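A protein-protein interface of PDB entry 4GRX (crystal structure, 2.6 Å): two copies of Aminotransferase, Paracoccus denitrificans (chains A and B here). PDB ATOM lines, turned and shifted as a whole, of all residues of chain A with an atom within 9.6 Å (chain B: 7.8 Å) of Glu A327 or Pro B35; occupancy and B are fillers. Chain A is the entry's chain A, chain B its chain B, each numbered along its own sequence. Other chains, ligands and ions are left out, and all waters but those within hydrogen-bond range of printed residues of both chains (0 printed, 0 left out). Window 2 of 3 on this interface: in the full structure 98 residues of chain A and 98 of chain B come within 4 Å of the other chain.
The backbone NH (N) of Met B34 sits at hydrogen-bond distance from the backbone carbonyl oxygen (O) of Glu A327 (3.3 Å).
The backbone NH (N) of Phe B31 lies within hydrogen-bond range of the backbone carbonyl oxygen (O) of Phe A329 (3.0 Å).
The side-chain hydroxyl (OG) of Ser B36 is in hydrogen-bond range of the side-chain carboxylate (OD2) of Asp B33 (2.7 Å).
CG1 of Val A323 touches CG of Met B34, at 3.9 Å.
OE2 of Glu A324 touches NE2 of His B38 (3.6 Å).
Thr B32 touches Glu A327 (O to O, 3.7 Å).
Glu A327 touches Asp B33 (O to CA, 3.8 Å).
CD of Glu A327 touches CG of Pro B35, 3.5 Å away.
OE2 of Glu A328 touches CD1 of Phe B31, at 3.3 Å.
Thr B32 touches Glu A328.
Glu A328 touches Asp B33 (OE1 to N, 3.98 Å).
Phe B31 touches Pro A330.
Glu A327 touches four residues of chain B.
Of the printed residues of chain A, Pro B35 touches Glu A327.
No residue of chain A comes within 4 Å of Ser B36.
Of the printed residues of chain B, Glu A328 touches Phe B31, Thr B32 and Asp B33.
Of the printed residues of chain A, Phe B31 touches Glu A328 (3.3 Å), Phe A329 (3.0 Å) and Pro A330 (3.7 Å).
Printed residues of chain B within 4 Å of Pro A330: Phe B31 (3.7 Å).
Of the printed residues of chain A, Thr B32 touches Glu A327 (3.7 Å) and Glu A328 (3.7 Å).
Of the printed residues of chain A, Met B34 touches Val A323 (3.9 Å) and Glu A327 (3.3 Å).
Ala A325 touches none of the printed residues of chain B.
Asn B417 touches none of the printed residues of chain A.
The nearest residue of chain B that does not touch Glu A327 is Ser B36 (7.1 Å).
The nearest residue of chain A that does not touch Pro B35 is Glu A328 (6.0 Å).
The nearest printed residue of chain A that does not touch Thr B32 is Phe A329 (4.6 Å).
Printed residues of chain B that touch a printed residue of chain A: Phe B31, Thr B32, Asp B33, Met B34, Pro B35 and His B38.
Hydrophobic or aromatic side chains of chain B within 4 Å of the printed part of chain A: Phe B31, Met B34, Pro B35 and His B38.
No position is printed for both chains.
Of the 11 pairs that touch across the chains among the printed residues, none has its exchanged pair printed and touching as well.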
ATOM      1  N   PHE A 142       8.744  16.221  -3.104  1.00  0.00           N
ATOM      2  CA  PHE A 142       7.469  16.929  -3.283  1.00  0.00           C
ATOM      3  C   PHE A 142       7.472  17.732  -4.587  1.00  0.00           C
ATOM      4  O   PHE A 142       6.570  17.594  -5.412  1.00  0.00           O
ATOM      5  CB  PHE A 142       7.244  17.842  -2.062  1.00  0.00           C
ATOM      6  CG  PHE A 142       6.042  18.742  -2.159  1.00  0.00           C
ATOM      7  CD1 PHE A 142       6.204  20.125  -2.288  1.00  0.00           C
ATOM      8  CD2 PHE A 142       4.749  18.225  -2.081  1.00  0.00           C
ATOM      9  CE1 PHE A 142       5.114  20.966  -2.366  1.00  0.00           C
ATOM     10  CE2 PHE A 142       3.652  19.063  -2.169  1.00  0.00           C
ATOM     11  CZ  PHE A 142       3.833  20.432  -2.314  1.00  0.00           C
ATOM     12  N   VAL A 319       8.165  25.948  -5.301  1.00  0.00           N
ATOM     13  CA  VAL A 319       7.621  25.289  -4.106  1.00  0.00           C
ATOM     14  C   VAL A 319       6.265  25.893  -3.743  1.00  0.00           C
ATOM     15  O   VAL A 319       5.289  25.164  -3.552  1.00  0.00           O
ATOM     16  CB  VAL A 319       8.581  25.368  -2.893  1.00  0.00           C
ATOM     17  CG1 VAL A 319       7.896  24.900  -1.620  1.00  0.00           C
ATOM     18  CG2 VAL A 319       9.831  24.548  -3.152  1.00  0.00           C
ATOM     19  N   GLU A 320       6.215  27.222  -3.673  1.00  0.00           N
ATOM     20  CA  GLU A 320       4.983  27.953  -3.378  1.00  0.00           C
ATOM     21  C   GLU A 320       3.839  27.545  -4.299  1.00  0.00           C
ATOM     22  O   GLU A 320       2.761  27.192  -3.813  1.00  0.00           O
ATOM     23  CB  GLU A 320       5.221  29.458  -3.462  1.00  0.00           C
ATOM     24  CG  GLU A 320       3.951  30.286  -3.439  1.00  0.00           C
ATOM     25  CD  GLU A 320       4.085  31.563  -4.246  1.00  0.00           C
ATOM     26  OE1 GLU A 320       4.835  32.469  -3.804  1.00  0.00           O
ATOM     27  OE2 GLU A 320       3.438  31.656  -5.319  1.00  0.00           O
ATOM     28  N   ALA A 321       4.067  27.593  -5.613  1.00  0.00           N
ATOM     29  CA  ALA A 321       3.060  27.172  -6.591  1.00  0.00           C
ATOM     30  C   ALA A 321       2.629  25.724  -6.363  1.00  0.00           C
ATOM     31  O   ALA A 321       1.431  25.421  -6.347  1.00  0.00           O
ATOM     32  CB  ALA A 321       3.575  27.349  -8.009  1.00  0.00           C
ATOM     33  N   ALA A 322       3.613  24.842  -6.171  1.00  0.00           N
ATOM     34  CA  ALA A 322       3.369  23.409  -5.973  1.00  0.00           C
ATOM     35  C   ALA A 322       2.456  23.145  -4.780  1.00  0.00           C
ATOM     36  O   ALA A 322       1.570  22.292  -4.855  1.00  0.00           O
ATOM     37  CB  ALA A 322       4.686  22.672  -5.811  1.00  0.00           C
ATOM     38  N   VAL A 323       2.684  23.896  -3.700  1.00  0.00           N
ATOM     39  CA  VAL A 323       1.890  23.853  -2.475  1.00  0.00           C
ATOM     40  C   VAL A 323       0.429  24.183  -2.749  1.00  0.00           C
ATOM     41  O   VAL A 323      -0.445  23.370  -2.444  1.00  0.00           O
ATOM     42  CB  VAL A 323       2.451  24.807  -1.385  1.00  0.00           C
ATOM     43  CG1 VAL A 323       1.478  24.971  -0.224  1.00  0.00           C
ATOM     44  CG2 VAL A 323       3.777  24.297  -0.858  1.00  0.00           C
ATOM     45  N   GLU A 324       0.169  25.350  -3.342  1.00  0.00           N
ATOM     46  CA  GLU A 324      -1.205  25.814  -3.591  1.00  0.00           C
ATOM     47  C   GLU A 324      -2.042  24.889  -4.477  1.00  0.00           C
ATOM     48  O   GLU A 324      -3.275  24.915  -4.400  1.00  0.00           O
ATOM     49  CB  GLU A 324      -1.230  27.255  -4.115  1.00  0.00           C
ATOM     50  CG  GLU A 324      -1.368  28.304  -3.018  1.00  0.00           C
ATOM     51  CD  GLU A 324      -0.549  29.552  -3.295  1.00  0.00           C
ATOM     52  OE1 GLU A 324      -0.908  30.308  -4.234  1.00  0.00           O
ATOM     53  OE2 GLU A 324       0.456  29.774  -2.567  1.00  0.00           O
ATOM     54  N   ALA A 325      -1.380  24.071  -5.296  1.00  0.00           N
ATOM     55  CA  ALA A 325      -2.074  23.065  -6.109  1.00  0.00           C
ATOM     56  C   ALA A 325      -2.724  21.979  -5.239  1.00  0.00           C
ATOM     57  O   ALA A 325      -3.681  21.332  -5.654  1.00  0.00           O
ATOM     58  CB  ALA A 325      -1.117  22.446  -7.119  1.00  0.00           C
ATOM     59  N   ILE A 326      -2.204  21.814  -4.023  1.00  0.00           N
ATOM     60  CA  ILE A 326      -2.541  20.700  -3.130  1.00  0.00           C
ATOM     61  C   ILE A 326      -3.175  21.211  -1.820  1.00  0.00           C
ATOM     62  O   ILE A 326      -3.941  20.497  -1.170  1.00  0.00           O
ATOM     63  CB  ILE A 326      -1.274  19.832  -2.889  1.00  0.00           C
ATOM     64  CG1 ILE A 326      -1.498  18.395  -3.370  1.00  0.00           C
ATOM     65  CG2 ILE A 326      -0.735  19.944  -1.463  1.00  0.00           C
ATOM     66  CD1 ILE A 326      -0.303  17.827  -4.115  1.00  0.00           C
ATOM     67  N   GLU A 327      -2.828  22.451  -1.459  1.00  0.00           N
ATOM     68  CA  GLU A 327      -3.456  23.255  -0.383  1.00  0.00           C
ATOM     69  C   GLU A 327      -2.840  23.199   1.022  1.00  0.00           C
ATOM     70  O   GLU A 327      -3.331  23.877   1.928  1.00  0.00           O
ATOM     71  CB  GLU A 327      -4.971  23.050  -0.320  1.00  0.00           C
ATOM     72  CG  GLU A 327      -5.712  23.804  -1.407  1.00  0.00           C
ATOM     73  CD  GLU A 327      -7.207  23.662  -1.294  1.00  0.00           C
ATOM     74  OE1 GLU A 327      -7.688  23.187  -0.246  1.00  0.00           O
ATOM     75  OE2 GLU A 327      -7.898  24.030  -2.259  1.00  0.00           O
ATOM     76  N   GLU A 328      -1.770  22.420   1.196  1.00  0.00           N
ATOM     77  CA  GLU A 328      -1.055  22.345   2.474  1.00  0.00           C
ATOM     78  C   GLU A 328       0.346  21.741   2.287  1.00  0.00           C
ATOM     79  O   GLU A 328       0.516  20.789   1.525  1.00  0.00           O
ATOM     80  CB  GLU A 328      -1.874  21.538   3.507  1.00  0.00           C
ATOM     81  CG  GLU A 328      -1.297  21.529   4.926  1.00  0.00           C
ATOM     82  CD  GLU A 328      -2.308  21.169   6.015  1.00  0.00           C
ATOM     83  OE1 GLU A 328      -3.509  21.480   5.859  1.00  0.00           O
ATOM     84  OE2 GLU A 328      -1.891  20.590   7.047  1.00  0.00           O
ATOM     85  N   PHE A 329       1.346  22.308   2.959  1.00  0.00           N
ATOM     86  CA  PHE A 329       2.655  21.657   3.069  1.00  0.00           C
ATOM     87  C   PHE A 329       2.638  20.767   4.322  1.00  0.00           C
ATOM     88  O   PHE A 329       2.915  21.245   5.426  1.00  0.00           O
ATOM     89  CB  PHE A 329       3.784  22.694   3.131  1.00  0.00           C
ATOM     90  CG  PHE A 329       5.174  22.100   3.152  1.00  0.00           C
ATOM     91  CD1 PHE A 329       5.676  21.398   2.054  1.00  0.00           C
ATOM     92  CD2 PHE A 329       6.006  22.275   4.259  1.00  0.00           C
ATOM     93  CE1 PHE A 329       6.963  20.867   2.072  1.00  0.00           C
ATOM     94  CE2 PHE A 329       7.294  21.750   4.275  1.00  0.00           C
ATOM     95  CZ  PHE A 329       7.771  21.040   3.183  1.00  0.00           C
ATOM     96  N   PRO A 330       2.292  19.468   4.159  1.00  0.00           N
ATOM     97  CA  PRO A 330       2.066  18.575   5.301  1.00  0.00           C
ATOM     98  C   PRO A 330       3.382  18.177   5.990  1.00  0.00           C
ATOM     99  O   PRO A 330       3.704  16.994   6.120  1.00  0.00           O
ATOM    100  CB  PRO A 330       1.377  17.359   4.668  1.00  0.00           C
ATOM    101  CG  PRO A 330       1.216  17.666   3.205  1.00  0.00           C
ATOM    102  CD  PRO A 330       2.206  18.734   2.885  1.00  0.00           C
ATOM    103  N   PHE B  31       2.161  22.733   7.907  1.00  0.00           N
ATOM    104  CA  PHE B  31       0.838  22.264   8.373  1.00  0.00           C
ATOM    105  C   PHE B  31      -0.255  23.363   8.440  1.00  0.00           C
ATOM    106  O   PHE B  31      -0.980  23.474   9.440  1.00  0.00           O
ATOM    107  CB  PHE B  31       0.958  21.504   9.714  1.00  0.00           C
ATOM    108  CG  PHE B  31       1.315  20.037   9.571  1.00  0.00           C
ATOM    109  CD1 PHE B  31       0.474  19.152   8.890  1.00  0.00           C
ATOM    110  CD2 PHE B  31       2.481  19.529  10.151  1.00  0.00           C
ATOM    111  CE1 PHE B  31       0.801  17.804   8.773  1.00  0.00           C
ATOM    112  CE2 PHE B  31       2.807  18.184  10.037  1.00  0.00           C
ATOM    113  CZ  PHE B  31       1.967  17.320   9.349  1.00  0.00           C
ATOM    114  N   THR B  32      -0.365  24.153   7.365  1.00  0.00           N
ATOM    115  CA  THR B  32      -1.268  25.320   7.291  1.00  0.00           C
ATOM    116  C   THR B  32      -2.133  25.327   6.019  1.00  0.00           C
ATOM    117  O   THR B  32      -1.609  25.238   4.899  1.00  0.00           O
ATOM    118  CB  THR B  32      -0.475  26.650   7.331  1.00  0.00           C
ATOM    119  OG1 THR B  32       0.329  26.708   8.515  1.00  0.00           O
ATOM    120  CG2 THR B  32      -1.415  27.868   7.286  1.00  0.00           C
ATOM    121  N   ASP B  33      -3.451  25.448   6.195  1.00  0.00           N
ATOM    122  CA  ASP B  33      -4.369  25.654   5.071  1.00  0.00           C
ATOM    123  C   ASP B  33      -4.035  26.976   4.378  1.00  0.00           C
ATOM    124  O   ASP B  33      -4.004  28.028   5.014  1.00  0.00           O
ATOM    125  CB  ASP B  33      -5.833  25.640   5.537  1.00  0.00           C
ATOM    126  CG  ASP B  33      -6.820  25.711   4.376  1.00  0.00           C
ATOM    127  OD1 ASP B  33      -6.878  24.756   3.578  1.00  0.00           O
ATOM    128  OD2 ASP B  33      -7.540  26.723   4.260  1.00  0.00           O
ATOM    129  N   MET B  34      -3.763  26.912   3.080  1.00  0.00           N
ATOM    130  CA  MET B  34      -3.431  28.113   2.317  1.00  0.00           C
ATOM    131  C   MET B  34      -4.659  28.930   1.852  1.00  0.00           C
ATOM    132  O   MET B  34      -4.599  30.169   1.858  1.00  0.00           O
ATOM    133  CB  MET B  34      -2.461  27.799   1.159  1.00  0.00           C
ATOM    134  CG  MET B  34      -1.088  27.283   1.599  1.00  0.00           C
ATOM    135  SD  MET B  34      -0.256  28.250   2.889  1.00  0.00           S
ATOM    136  CE  MET B  34       0.236  29.727   1.997  1.00  0.00           C
ATOM    137  N   PRO B  35      -5.772  28.252   1.448  1.00  0.00           N
ATOM    138  CA  PRO B  35      -7.018  28.986   1.159  1.00  0.00           C
ATOM    139  C   PRO B  35      -7.599  29.854   2.290  1.00  0.00           C
ATOM    140  O   PRO B  35      -8.320  30.810   1.993  1.00  0.00           O
ATOM    141  CB  PRO B  35      -8.000  27.870   0.786  1.00  0.00           C
ATOM    142  CG  PRO B  35      -7.136  26.837   0.162  1.00  0.00           C
ATOM    143  CD  PRO B  35      -5.859  26.857   0.962  1.00  0.00           C
ATOM    144  N   SER B  36      -7.306  29.534   3.554  1.00  0.00           N
ATOM    145  CA  SER B  36      -7.837  30.323   4.685  1.00  0.00           C
ATOM    146  C   SER B  36      -6.809  31.189   5.452  1.00  0.00           C
ATOM    147  O   SER B  36      -7.193  32.043   6.255  1.00  0.00           O
ATOM    148  CB  SER B  36      -8.667  29.456   5.647  1.00  0.00           C
ATOM    149  OG  SER B  36      -7.869  28.500   6.310  1.00  0.00           O
ATOM    150  N   VAL B  37      -5.518  30.976   5.204  1.00  0.00           N
ATOM    151  CA  VAL B  37      -4.486  31.891   5.708  1.00  0.00           C
ATOM    152  C   VAL B  37      -4.265  33.040   4.711  1.00  0.00           C
ATOM    153  O   VAL B  37      -3.828  34.125   5.100  1.00  0.00           O
ATOM    154  CB  VAL B  37      -3.162  31.161   6.078  1.00  0.00           C
ATOM    155  CG1 VAL B  37      -2.323  30.845   4.843  1.00  0.00           C
ATOM    156  CG2 VAL B  37      -2.357  31.983   7.076  1.00  0.00           C
ATOM    157  N   HIS B  38      -4.564  32.780   3.433  1.00  0.00           N
ATOM    158  CA  HIS B  38      -4.652  33.831   2.412  1.00  0.00           C
ATOM    159  C   HIS B  38      -5.940  34.597   2.576  1.00  0.00           C
ATOM    160  O   HIS B  38      -5.979  35.805   2.343  1.00  0.00           O
ATOM    161  CB  HIS B  38      -4.544  33.264   0.986  1.00  0.00           C
ATOM    162  CG  HIS B  38      -3.132  32.877   0.571  1.00  0.00           C
ATOM    163  ND1 HIS B  38      -2.051  33.641   0.844  1.00  0.00           N
ATOM    164  CD2 HIS B  38      -2.660  31.779  -0.144  1.00  0.00           C
ATOM    165  CE1 HIS B  38      -0.945  33.051   0.351  1.00  0.00           C
ATOM    166  NE2 HIS B  38      -1.317  31.914  -0.254  1.00  0.00           N
ATOM    167  N   GLN B  39      -7.001  33.897   2.984  1.00  0.00           N
ATOM    168  CA  GLN B  39      -8.320  34.495   3.220  1.00  0.00           C
ATOM    169  C   GLN B  39      -8.366  35.341   4.502  1.00  0.00           C
ATOM    170  O   GLN B  39      -8.610  36.548   4.444  1.00  0.00           O
ATOM    171  CB  GLN B  39      -9.414  33.402   3.198  1.00  0.00           C
ATOM    172  CG  GLN B  39     -10.684  33.673   4.002  1.00  0.00           C
ATOM    173  CD  GLN B  39     -11.519  34.824   3.459  1.00  0.00           C
ATOM    174  OE1 GLN B  39     -11.662  34.993   2.242  1.00  0.00           O
ATOM    175  NE2 GLN B  39     -12.088  35.619   4.366  1.00  0.00           N
ATOM    176  N   ARG B  40      -8.136  34.704   5.650  1.00  0.00           N
ATOM    177  CA  ARG B  40      -8.185  35.375   6.951  1.00  0.00           C
ATOM    178  C   ARG B  40      -6.798  35.896   7.292  1.00  0.00           C
ATOM    179  O   ARG B  40      -5.816  35.479   6.678  1.00  0.00           O
ATOM    180  CB  ARG B  40      -8.646  34.400   8.036  1.00  0.00           C
ATOM    181  CG  ARG B  40      -9.949  33.672   7.730  1.00  0.00           C
ATOM    182  CD  ARG B  40     -10.069  32.386   8.533  1.00  0.00           C
ATOM    183  NE  ARG B  40      -9.958  32.626   9.973  1.00  0.00           N
ATOM    184  CZ  ARG B  40     -10.986  32.788  10.804  1.00  0.00           C
ATOM    185  NH1 ARG B  40     -12.236  32.727  10.360  1.00  0.00           N
ATOM    186  NH2 ARG B  40     -10.759  33.002  12.093  1.00  0.00           N
ATOM    187  N   SER B 410     -16.226  21.233   4.265  1.00  0.00           N
ATOM    188  CA  SER B 410     -15.123  21.601   5.182  1.00  0.00           C
ATOM    189  C   SER B 410     -15.634  21.828   6.592  1.00  0.00           C
ATOM    190  O   SER B 410     -15.245  22.784   7.270  1.00  0.00           O
ATOM    191  CB  SER B 410     -14.379  22.847   4.697  1.00  0.00           C
ATOM    192  OG  SER B 410     -14.007  22.745   3.340  1.00  0.00           O
ATOM    193  N   ASN B 417     -12.628  27.674  12.551  1.00  0.00           N
ATOM    194  CA  ASN B 417     -12.694  29.096  12.204  1.00  0.00           C
ATOM    195  C   ASN B 417     -13.661  29.928  13.051  1.00  0.00           C
ATOM    196  O   ASN B 417     -13.285  30.999  13.534  1.00  0.00           O
ATOM    197  CB  ASN B 417     -12.974  29.291  10.706  1.00  0.00           C
ATOM    198  CG  ASN B 417     -11.710  29.241   9.860  1.00  0.00           C
ATOM    199  OD1 ASN B 417     -10.599  29.287  10.381  1.00  0.00           O
ATOM    200  ND2 ASN B 417     -11.877  29.153   8.546  1.00  0.00           N
